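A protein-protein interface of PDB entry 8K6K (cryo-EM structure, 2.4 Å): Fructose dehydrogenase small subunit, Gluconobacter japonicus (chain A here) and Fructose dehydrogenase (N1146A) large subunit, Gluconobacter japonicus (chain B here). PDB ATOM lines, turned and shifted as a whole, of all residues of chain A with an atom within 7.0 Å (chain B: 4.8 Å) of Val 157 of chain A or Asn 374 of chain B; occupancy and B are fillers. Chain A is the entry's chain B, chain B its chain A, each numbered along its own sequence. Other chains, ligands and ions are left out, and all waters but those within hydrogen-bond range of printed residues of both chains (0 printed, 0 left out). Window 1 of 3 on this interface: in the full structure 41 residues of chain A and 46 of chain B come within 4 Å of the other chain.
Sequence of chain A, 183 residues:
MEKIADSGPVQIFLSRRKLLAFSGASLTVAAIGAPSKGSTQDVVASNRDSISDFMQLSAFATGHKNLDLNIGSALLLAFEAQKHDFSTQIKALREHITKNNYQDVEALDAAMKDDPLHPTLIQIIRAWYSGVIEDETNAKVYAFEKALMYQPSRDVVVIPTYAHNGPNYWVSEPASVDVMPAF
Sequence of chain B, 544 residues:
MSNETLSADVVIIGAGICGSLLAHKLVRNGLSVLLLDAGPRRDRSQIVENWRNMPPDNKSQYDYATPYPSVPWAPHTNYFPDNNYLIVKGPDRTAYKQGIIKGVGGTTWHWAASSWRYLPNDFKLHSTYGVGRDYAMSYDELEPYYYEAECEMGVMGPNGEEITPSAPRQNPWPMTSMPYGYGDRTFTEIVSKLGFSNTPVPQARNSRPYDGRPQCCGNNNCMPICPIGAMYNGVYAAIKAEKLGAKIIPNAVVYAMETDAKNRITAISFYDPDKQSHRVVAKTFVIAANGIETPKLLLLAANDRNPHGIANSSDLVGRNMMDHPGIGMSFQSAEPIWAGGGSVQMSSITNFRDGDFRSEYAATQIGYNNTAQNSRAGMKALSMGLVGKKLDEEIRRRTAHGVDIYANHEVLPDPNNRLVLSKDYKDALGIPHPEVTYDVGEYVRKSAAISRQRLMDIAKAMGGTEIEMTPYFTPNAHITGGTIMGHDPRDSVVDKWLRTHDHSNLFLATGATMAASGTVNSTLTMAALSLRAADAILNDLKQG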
ATOM      1  N   MET A 149      31.871  17.144  19.468  1.00  0.00           N
ATOM      2  CA  MET A 149      31.063  16.848  20.644  1.00  0.00           C
ATOM      3  C   MET A 149      29.710  16.248  20.295  1.00  0.00           C
ATOM      4  O   MET A 149      29.019  15.757  21.193  1.00  0.00           O
ATOM      5  CB  MET A 149      30.862  18.106  21.491  1.00  0.00           C
ATOM      6  CG  MET A 149      29.994  19.169  20.855  1.00  0.00           C
ATOM      7  SD  MET A 149      29.753  20.574  21.951  1.00  0.00           S
ATOM      8  CE  MET A 149      28.185  21.185  21.364  1.00  0.00           C
ATOM      9  N   TYR A 150      29.315  16.277  19.026  1.00  0.00           N
ATOM     10  CA  TYR A 150      28.081  15.641  18.591  1.00  0.00           C
ATOM     11  C   TYR A 150      28.291  14.215  18.108  1.00  0.00           C
ATOM     12  O   TYR A 150      27.309  13.496  17.906  1.00  0.00           O
ATOM     13  CB  TYR A 150      27.433  16.461  17.474  1.00  0.00           C
ATOM     14  CG  TYR A 150      26.957  17.822  17.916  1.00  0.00           C
ATOM     15  CD1 TYR A 150      25.899  17.953  18.799  1.00  0.00           C
ATOM     16  CD2 TYR A 150      27.567  18.974  17.451  1.00  0.00           C
ATOM     17  CE1 TYR A 150      25.462  19.191  19.206  1.00  0.00           C
ATOM     18  CE2 TYR A 150      27.137  20.217  17.852  1.00  0.00           C
ATOM     19  CZ  TYR A 150      26.084  20.320  18.729  1.00  0.00           C
ATOM     20  OH  TYR A 150      25.651  21.560  19.134  1.00  0.00           O
ATOM     21  N   GLN A 151      29.536  13.793  17.928  1.00  0.00           N
ATOM     22  CA  GLN A 151      29.880  12.491  17.370  1.00  0.00           C
ATOM     23  C   GLN A 151      29.732  11.331  18.355  1.00  0.00           C
ATOM     24  O   GLN A 151      29.315  10.244  17.937  1.00  0.00           O
ATOM     25  CB  GLN A 151      31.306  12.528  16.819  1.00  0.00           C
ATOM     26  CG  GLN A 151      31.620  13.772  16.019  1.00  0.00           C
ATOM     27  CD  GLN A 151      30.633  14.005  14.902  1.00  0.00           C
ATOM     28  OE1 GLN A 151      30.432  13.143  14.051  1.00  0.00           O
ATOM     29  NE2 GLN A 151      30.009  15.174  14.896  1.00  0.00           N
ATOM     30  N   SER A 153      27.476  10.663  20.276  1.00  0.00           N
ATOM     31  CA  SER A 153      26.074  10.271  20.363  1.00  0.00           C
ATOM     32  C   SER A 153      25.368  10.330  19.014  1.00  0.00           C
ATOM     33  O   SER A 153      24.136  10.342  18.967  1.00  0.00           O
ATOM     34  CB  SER A 153      25.341  11.150  21.372  1.00  0.00           C
ATOM     35  OG  SER A 153      25.731  12.504  21.240  1.00  0.00           O
ATOM     36  N   ARG A 154      26.123  10.368  17.915  1.00  0.00           N
ATOM     37  CA  ARG A 154      25.504  10.463  16.598  1.00  0.00           C
ATOM     38  C   ARG A 154      24.664   9.236  16.280  1.00  0.00           C
ATOM     39  O   ARG A 154      23.639   9.346  15.599  1.00  0.00           O
ATOM     40  CB  ARG A 154      26.573  10.652  15.525  1.00  0.00           C
ATOM     41  CG  ARG A 154      26.783  12.087  15.108  1.00  0.00           C
ATOM     42  CD  ARG A 154      27.430  12.166  13.744  1.00  0.00           C
ATOM     43  NE  ARG A 154      26.463  12.470  12.699  1.00  0.00           N
ATOM     44  CZ  ARG A 154      26.697  13.285  11.682  1.00  0.00           C
ATOM     45  NH1 ARG A 154      27.861  13.893  11.539  1.00  0.00           N
ATOM     46  NH2 ARG A 154      25.739  13.493  10.783  1.00  0.00           N
ATOM     47  N   ASP A 155      25.078   8.061  16.758  1.00  0.00           N
ATOM     48  CA  ASP A 155      24.356   6.837  16.443  1.00  0.00           C
ATOM     49  C   ASP A 155      22.991   6.772  17.115  1.00  0.00           C
ATOM     50  O   ASP A 155      22.161   5.950  16.718  1.00  0.00           O
ATOM     51  CB  ASP A 155      25.190   5.620  16.839  1.00  0.00           C
ATOM     52  CG  ASP A 155      25.497   5.582  18.317  1.00  0.00           C
ATOM     53  OD1 ASP A 155      25.626   6.663  18.925  1.00  0.00           O
ATOM     54  OD2 ASP A 155      25.613   4.472  18.873  1.00  0.00           O
ATOM     55  N   VAL A 156      22.738   7.611  18.116  1.00  0.00           N
ATOM     56  CA  VAL A 156      21.458   7.599  18.813  1.00  0.00           C
ATOM     57  C   VAL A 156      20.795   8.965  18.723  1.00  0.00           C
ATOM     58  O   VAL A 156      19.698   9.101  18.171  1.00  0.00           O
ATOM     59  CB  VAL A 156      21.626   7.180  20.284  1.00  0.00           C
ATOM     60  CG1 VAL A 156      20.270   7.031  20.937  1.00  0.00           C
ATOM     61  CG2 VAL A 156      22.413   5.889  20.386  1.00  0.00           C
ATOM     62  N   VAL A 157      21.450   9.979  19.265  1.00  0.00           N
ATOM     63  CA  VAL A 157      20.861  11.305  19.406  1.00  0.00           C
ATOM     64  C   VAL A 157      20.982  12.059  18.092  1.00  0.00           C
ATOM     65  O   VAL A 157      22.015  12.012  17.417  1.00  0.00           O
ATOM     66  CB  VAL A 157      21.527  12.079  20.556  1.00  0.00           C
ATOM     67  CG1 VAL A 157      20.788  13.374  20.816  1.00  0.00           C
ATOM     68  CG2 VAL A 157      21.557  11.230  21.805  1.00  0.00           C
ATOM     69  N   VAL A 158      19.919  12.760  17.733  1.00  0.00           N
ATOM     70  CA  VAL A 158      19.881  13.547  16.510  1.00  0.00           C
ATOM     71  C   VAL A 158      20.668  14.835  16.709  1.00  0.00           C
ATOM     72  O   VAL A 158      20.614  15.460  17.773  1.00  0.00           O
ATOM     73  CB  VAL A 158      18.422  13.839  16.114  1.00  0.00           C
ATOM     74  CG1 VAL A 158      17.676  14.471  17.272  1.00  0.00           C
ATOM     75  CG2 VAL A 158      18.359  14.737  14.898  1.00  0.00           C
ATOM     76  N   ILE A 159      21.425  15.227  15.690  1.00  0.00           N
ATOM     77  CA  ILE A 159      21.931  16.591  15.613  1.00  0.00           C
ATOM     78  C   ILE A 159      20.771  17.411  15.066  1.00  0.00           C
ATOM     79  O   ILE A 159      20.372  17.212  13.911  1.00  0.00           O
ATOM     80  CB  ILE A 159      23.188  16.683  14.737  1.00  0.00           C
ATOM     81  CG1 ILE A 159      24.248  15.706  15.241  1.00  0.00           C
ATOM     82  CG2 ILE A 159      23.731  18.095  14.732  1.00  0.00           C
ATOM     83  CD1 ILE A 159      25.483  15.653  14.390  1.00  0.00           C
ATOM     84  N   PRO A 160      20.218  18.345  15.846  1.00  0.00           N
ATOM     85  CA  PRO A 160      18.833  18.790  15.626  1.00  0.00           C
ATOM     86  C   PRO A 160      18.423  19.138  14.200  1.00  0.00           C
ATOM     87  O   PRO A 160      17.544  18.474  13.646  1.00  0.00           O
ATOM     88  CB  PRO A 160      18.735  20.013  16.539  1.00  0.00           C
ATOM     89  CG  PRO A 160      19.611  19.657  17.683  1.00  0.00           C
ATOM     90  CD  PRO A 160      20.764  18.872  17.108  1.00  0.00           C
ATOM     91  N   HIS A 164      17.719  12.307  11.380  1.00  0.00           N
ATOM     92  CA  HIS A 164      18.097  10.906  11.449  1.00  0.00           C
ATOM     93  C   HIS A 164      17.294  10.128  10.406  1.00  0.00           C
ATOM     94  O   HIS A 164      16.454  10.680   9.692  1.00  0.00           O
ATOM     95  CB  HIS A 164      17.861  10.365  12.855  1.00  0.00           C
ATOM     96  CG  HIS A 164      19.105   9.929  13.562  1.00  0.00           C
ATOM     97  ND1 HIS A 164      19.281   8.645  14.029  1.00  0.00           N
ATOM     98  CD2 HIS A 164      20.228  10.607  13.893  1.00  0.00           C
ATOM     99  CE1 HIS A 164      20.462   8.549  14.613  1.00  0.00           C
ATOM    100  NE2 HIS A 164      21.057   9.726  14.543  1.00  0.00           N
ATOM    101  N   TYR A 169      11.983   6.992  13.099  1.00  0.00           N
ATOM    102  CA  TYR A 169      13.103   6.154  13.510  1.00  0.00           C
ATOM    103  C   TYR A 169      13.137   5.907  15.011  1.00  0.00           C
ATOM    104  O   TYR A 169      13.715   4.907  15.448  1.00  0.00           O
ATOM    105  CB  TYR A 169      14.422   6.788  13.067  1.00  0.00           C
ATOM    106  CG  TYR A 169      14.816   8.009  13.867  1.00  0.00           C
ATOM    107  CD1 TYR A 169      14.381   9.272  13.497  1.00  0.00           C
ATOM    108  CD2 TYR A 169      15.623   7.899  14.990  1.00  0.00           C
ATOM    109  CE1 TYR A 169      14.734  10.386  14.225  1.00  0.00           C
ATOM    110  CE2 TYR A 169      15.977   9.006  15.723  1.00  0.00           C
ATOM    111  CZ  TYR A 169      15.531  10.247  15.337  1.00  0.00           C
ATOM    112  OH  TYR A 169      15.888  11.356  16.066  1.00  0.00           O
ATOM    113  N   TRP B 338      18.110   9.279  26.853  1.00  0.00           N
ATOM    114  CA  TRP B 338      18.283   9.492  25.417  1.00  0.00           C
ATOM    115  C   TRP B 338      17.234  10.461  24.867  1.00  0.00           C
ATOM    116  O   TRP B 338      16.436  10.127  23.990  1.00  0.00           O
ATOM    117  CB  TRP B 338      18.245   8.161  24.661  1.00  0.00           C
ATOM    118  CG  TRP B 338      19.399   7.243  24.931  1.00  0.00           C
ATOM    119  CD1 TRP B 338      19.351   6.036  25.562  1.00  0.00           C
ATOM    120  CD2 TRP B 338      20.765   7.441  24.553  1.00  0.00           C
ATOM    121  NE1 TRP B 338      20.601   5.476  25.612  1.00  0.00           N
ATOM    122  CE2 TRP B 338      21.488   6.319  24.998  1.00  0.00           C
ATOM    123  CE3 TRP B 338      21.450   8.461  23.889  1.00  0.00           C
ATOM    124  CZ2 TRP B 338      22.858   6.187  24.796  1.00  0.00           C
ATOM    125  CZ3 TRP B 338      22.810   8.328  23.690  1.00  0.00           C
ATOM    126  CH2 TRP B 338      23.499   7.200  24.142  1.00  0.00           C
ATOM    127  N   ALA B 339      17.246  11.677  25.403  1.00  0.00           N
ATOM    128  CA  ALA B 339      16.333  12.706  24.928  1.00  0.00           C
ATOM    129  C   ALA B 339      16.680  13.109  23.501  1.00  0.00           C
ATOM    130  O   ALA B 339      17.853  13.211  23.137  1.00  0.00           O
ATOM    131  CB  ALA B 339      16.382  13.926  25.844  1.00  0.00           C
ATOM    132  N   ALA B 372      17.156  17.474  22.481  1.00  0.00           N
ATOM    133  CA  ALA B 372      18.389  16.704  22.532  1.00  0.00           C
ATOM    134  C   ALA B 372      19.400  17.375  23.452  1.00  0.00           C
ATOM    135  O   ALA B 372      19.539  18.600  23.463  1.00  0.00           O
ATOM    136  CB  ALA B 372      18.972  16.548  21.130  1.00  0.00           C
ATOM    137  N   GLN B 373      20.110  16.561  24.230  1.00  0.00           N
ATOM    138  CA  GLN B 373      21.054  17.055  25.221  1.00  0.00           C
ATOM    139  C   GLN B 373      22.498  16.975  24.747  1.00  0.00           C
ATOM    140  O   GLN B 373      23.414  17.098  25.565  1.00  0.00           O
ATOM    141  CB  GLN B 373      20.890  16.289  26.532  1.00  0.00           C
ATOM    142  CG  GLN B 373      19.531  16.457  27.172  1.00  0.00           C
ATOM    143  CD  GLN B 373      19.548  17.456  28.305  1.00  0.00           C
ATOM    144  OE1 GLN B 373      20.534  17.575  29.027  1.00  0.00           O
ATOM    145  NE2 GLN B 373      18.455  18.188  28.461  1.00  0.00           N
ATOM    146  N   ASN B 374      22.723  16.762  23.449  1.00  0.00           N
ATOM    147  CA  ASN B 374      24.091  16.631  22.957  1.00  0.00           C
ATOM    148  C   ASN B 374      24.869  17.932  23.112  1.00  0.00           C
ATOM    149  O   ASN B 374      26.044  17.912  23.490  1.00  0.00           O
ATOM    150  CB  ASN B 374      24.087  16.171  21.501  1.00  0.00           C
ATOM    151  CG  ASN B 374      22.928  16.733  20.715  1.00  0.00           C
ATOM    152  OD1 ASN B 374      22.302  17.707  21.124  1.00  0.00           O
ATOM    153  ND2 ASN B 374      22.636  16.121  19.578  1.00  0.00           N
ATOM    154  N   SER B 375      24.238  19.072  22.825  1.00  0.00           N
ATOM    155  CA  SER B 375      24.913  20.355  23.004  1.00  0.00           C
ATOM    156  C   SER B 375      25.218  20.611  24.474  1.00  0.00           C
ATOM    157  O   SER B 375      26.335  21.006  24.833  1.00  0.00           O
ATOM    158  CB  SER B 375      24.055  21.481  22.431  1.00  0.00           C
ATOM    159  OG  SER B 375      24.081  21.474  21.016  1.00  0.00           O
ATOM    160  N   ARG B 376      24.229  20.386  25.338  1.00  0.00           N
ATOM    161  CA  ARG B 376      24.428  20.567  26.771  1.00  0.00           C
ATOM    162  C   ARG B 376      25.502  19.631  27.300  1.00  0.00           C
ATOM    163  O   ARG B 376      26.379  20.048  28.065  1.00  0.00           O
ATOM    164  CB  ARG B 376      23.107  20.345  27.504  1.00  0.00           C
ATOM    165  CG  ARG B 376      23.223  20.244  29.008  1.00  0.00           C
ATOM    166  CD  ARG B 376      22.843  21.553  29.665  1.00  0.00           C
ATOM    167  NE  ARG B 376      21.738  22.199  28.972  1.00  0.00           N
ATOM    168  CZ  ARG B 376      20.466  22.105  29.333  1.00  0.00           C
ATOM    169  NH1 ARG B 376      20.097  21.392  30.383  1.00  0.00           N
ATOM    170  NH2 ARG B 376      19.541  22.741  28.621  1.00  0.00           N
ATOM    171  N   ALA B 377      25.456  18.360  26.894  1.00  0.00           N
ATOM    172  CA  ALA B 377      26.453  17.398  27.345  1.00  0.00           C
ATOM    173  C   ALA B 377      27.846  17.782  26.875  1.00  0.00           C
ATOM    174  O   ALA B 377      28.810  17.709  27.645  1.00  0.00           O
ATOM    175  CB  ALA B 377      26.096  16.002  26.847  1.00  0.00           C
ATOM    176  N   GLY B 378      27.972  18.192  25.614  1.00  0.00           N
ATOM    177  CA  GLY B 378      29.274  18.576  25.101  1.00  0.00           C
ATOM    178  C   GLY B 378      29.847  19.774  25.828  1.00  0.00           C
ATOM    179  O   GLY B 378      31.016  19.778  26.221  1.00  0.00           O
ATOM    180  N   THR B 399      24.830  13.052  27.479  1.00  0.00           N
ATOM    181  CA  THR B 399      23.745  13.174  26.513  1.00  0.00           C
ATOM    182  C   THR B 399      22.756  12.023  26.631  1.00  0.00           C
ATOM    183  O   THR B 399      21.587  12.178  26.263  1.00  0.00           O
ATOM    184  CB  THR B 399      24.296  13.261  25.088  1.00  0.00           C
ATOM    185  OG1 THR B 399      23.225  13.520  24.176  1.00  0.00           O
ATOM    186  CG2 THR B 399      24.955  11.973  24.697  1.00  0.00           C
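The side-chain amide nitrogen of Asn 374 of chain B is in hydrogen-bond range of the backbone carbonyl oxygen of Val 158 of chain A (2.8 Å). The side-chain hydroxyl (OG) of Ser 375 of chain B sits at hydrogen-bond distance from the side-chain hydroxyl (OH) of Tyr 150 of chain A (2.5 Å).
N of Asn 374 of chain B sits at hydrogen-bond distance from OG1 of Thr 399 of chain B, at 3.4 Å.
Among the printed residues, pairs that only touch across the chains: Ser 153 of chain A with Thr 399 of chain B (3.4 Å), Val 157 of chain A with Trp 338 of chain B (3.5 Å), Val 156 of chain A with Trp 338 of chain B (3.5 Å), Val 157 of chain A with Asn 374 of chain B (3.5 Å), Val 157 of chain A with Ala 372 of chain B (3.7 Å), Val 157 of chain A with Thr 399 of chain B (3.7 Å), Tyr 150 of chain A with Asn 374 of chain B (3.7 Å), Val 157 of chain A with Ala 339 of chain B (3.7 Å), Met 149 of chain A with Ser 375 of chain B (3.8 Å), Met 149 of chain A with Gly 378 of chain B (3.8 Å) and Val 158 of chain A with Ala 372 of chain B (3.9 Å).
Of chain B, only Trp 338 (3.5 Å), Ala 339 (3.7 Å), Ala 372 (3.7 Å), Asn 374 (3.5 Å) and Thr 399 (3.7 Å) come within 4 Å of Val 157 of chain A. Of chain A, only Tyr 150 (3.7 Å), Val 157 (3.5 Å) and Val 158 (2.8 Å) come within 4 Å of Asn 374 of chain B. Of the printed residues of chain B, Tyr 150 of chain A touches Asn 374 and Ser 375. Of the printed residues of chain A, Trp 338 of chain B touches Val 156 (3.5 Å) and Val 157 (3.5 Å). The nearest printed residue of chain B that does not touch Met 149 of chain A is Asn 374 of chain B (4.3 Å).
Hydrophobic or aromatic side chains of chain A that line the printed part of chain B: Met 149, Tyr 150, Val 156 and Val 157. Printed residues of chain B that touch a printed residue of chain A: Trp 338, Ala 339, Ala 372, Asn 374, Ser 375, Gly 378 and Thr 399. Hydrophobic or aromatic side chains of chain B that line the printed part of chain A: Trp 338 and Ala 372.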
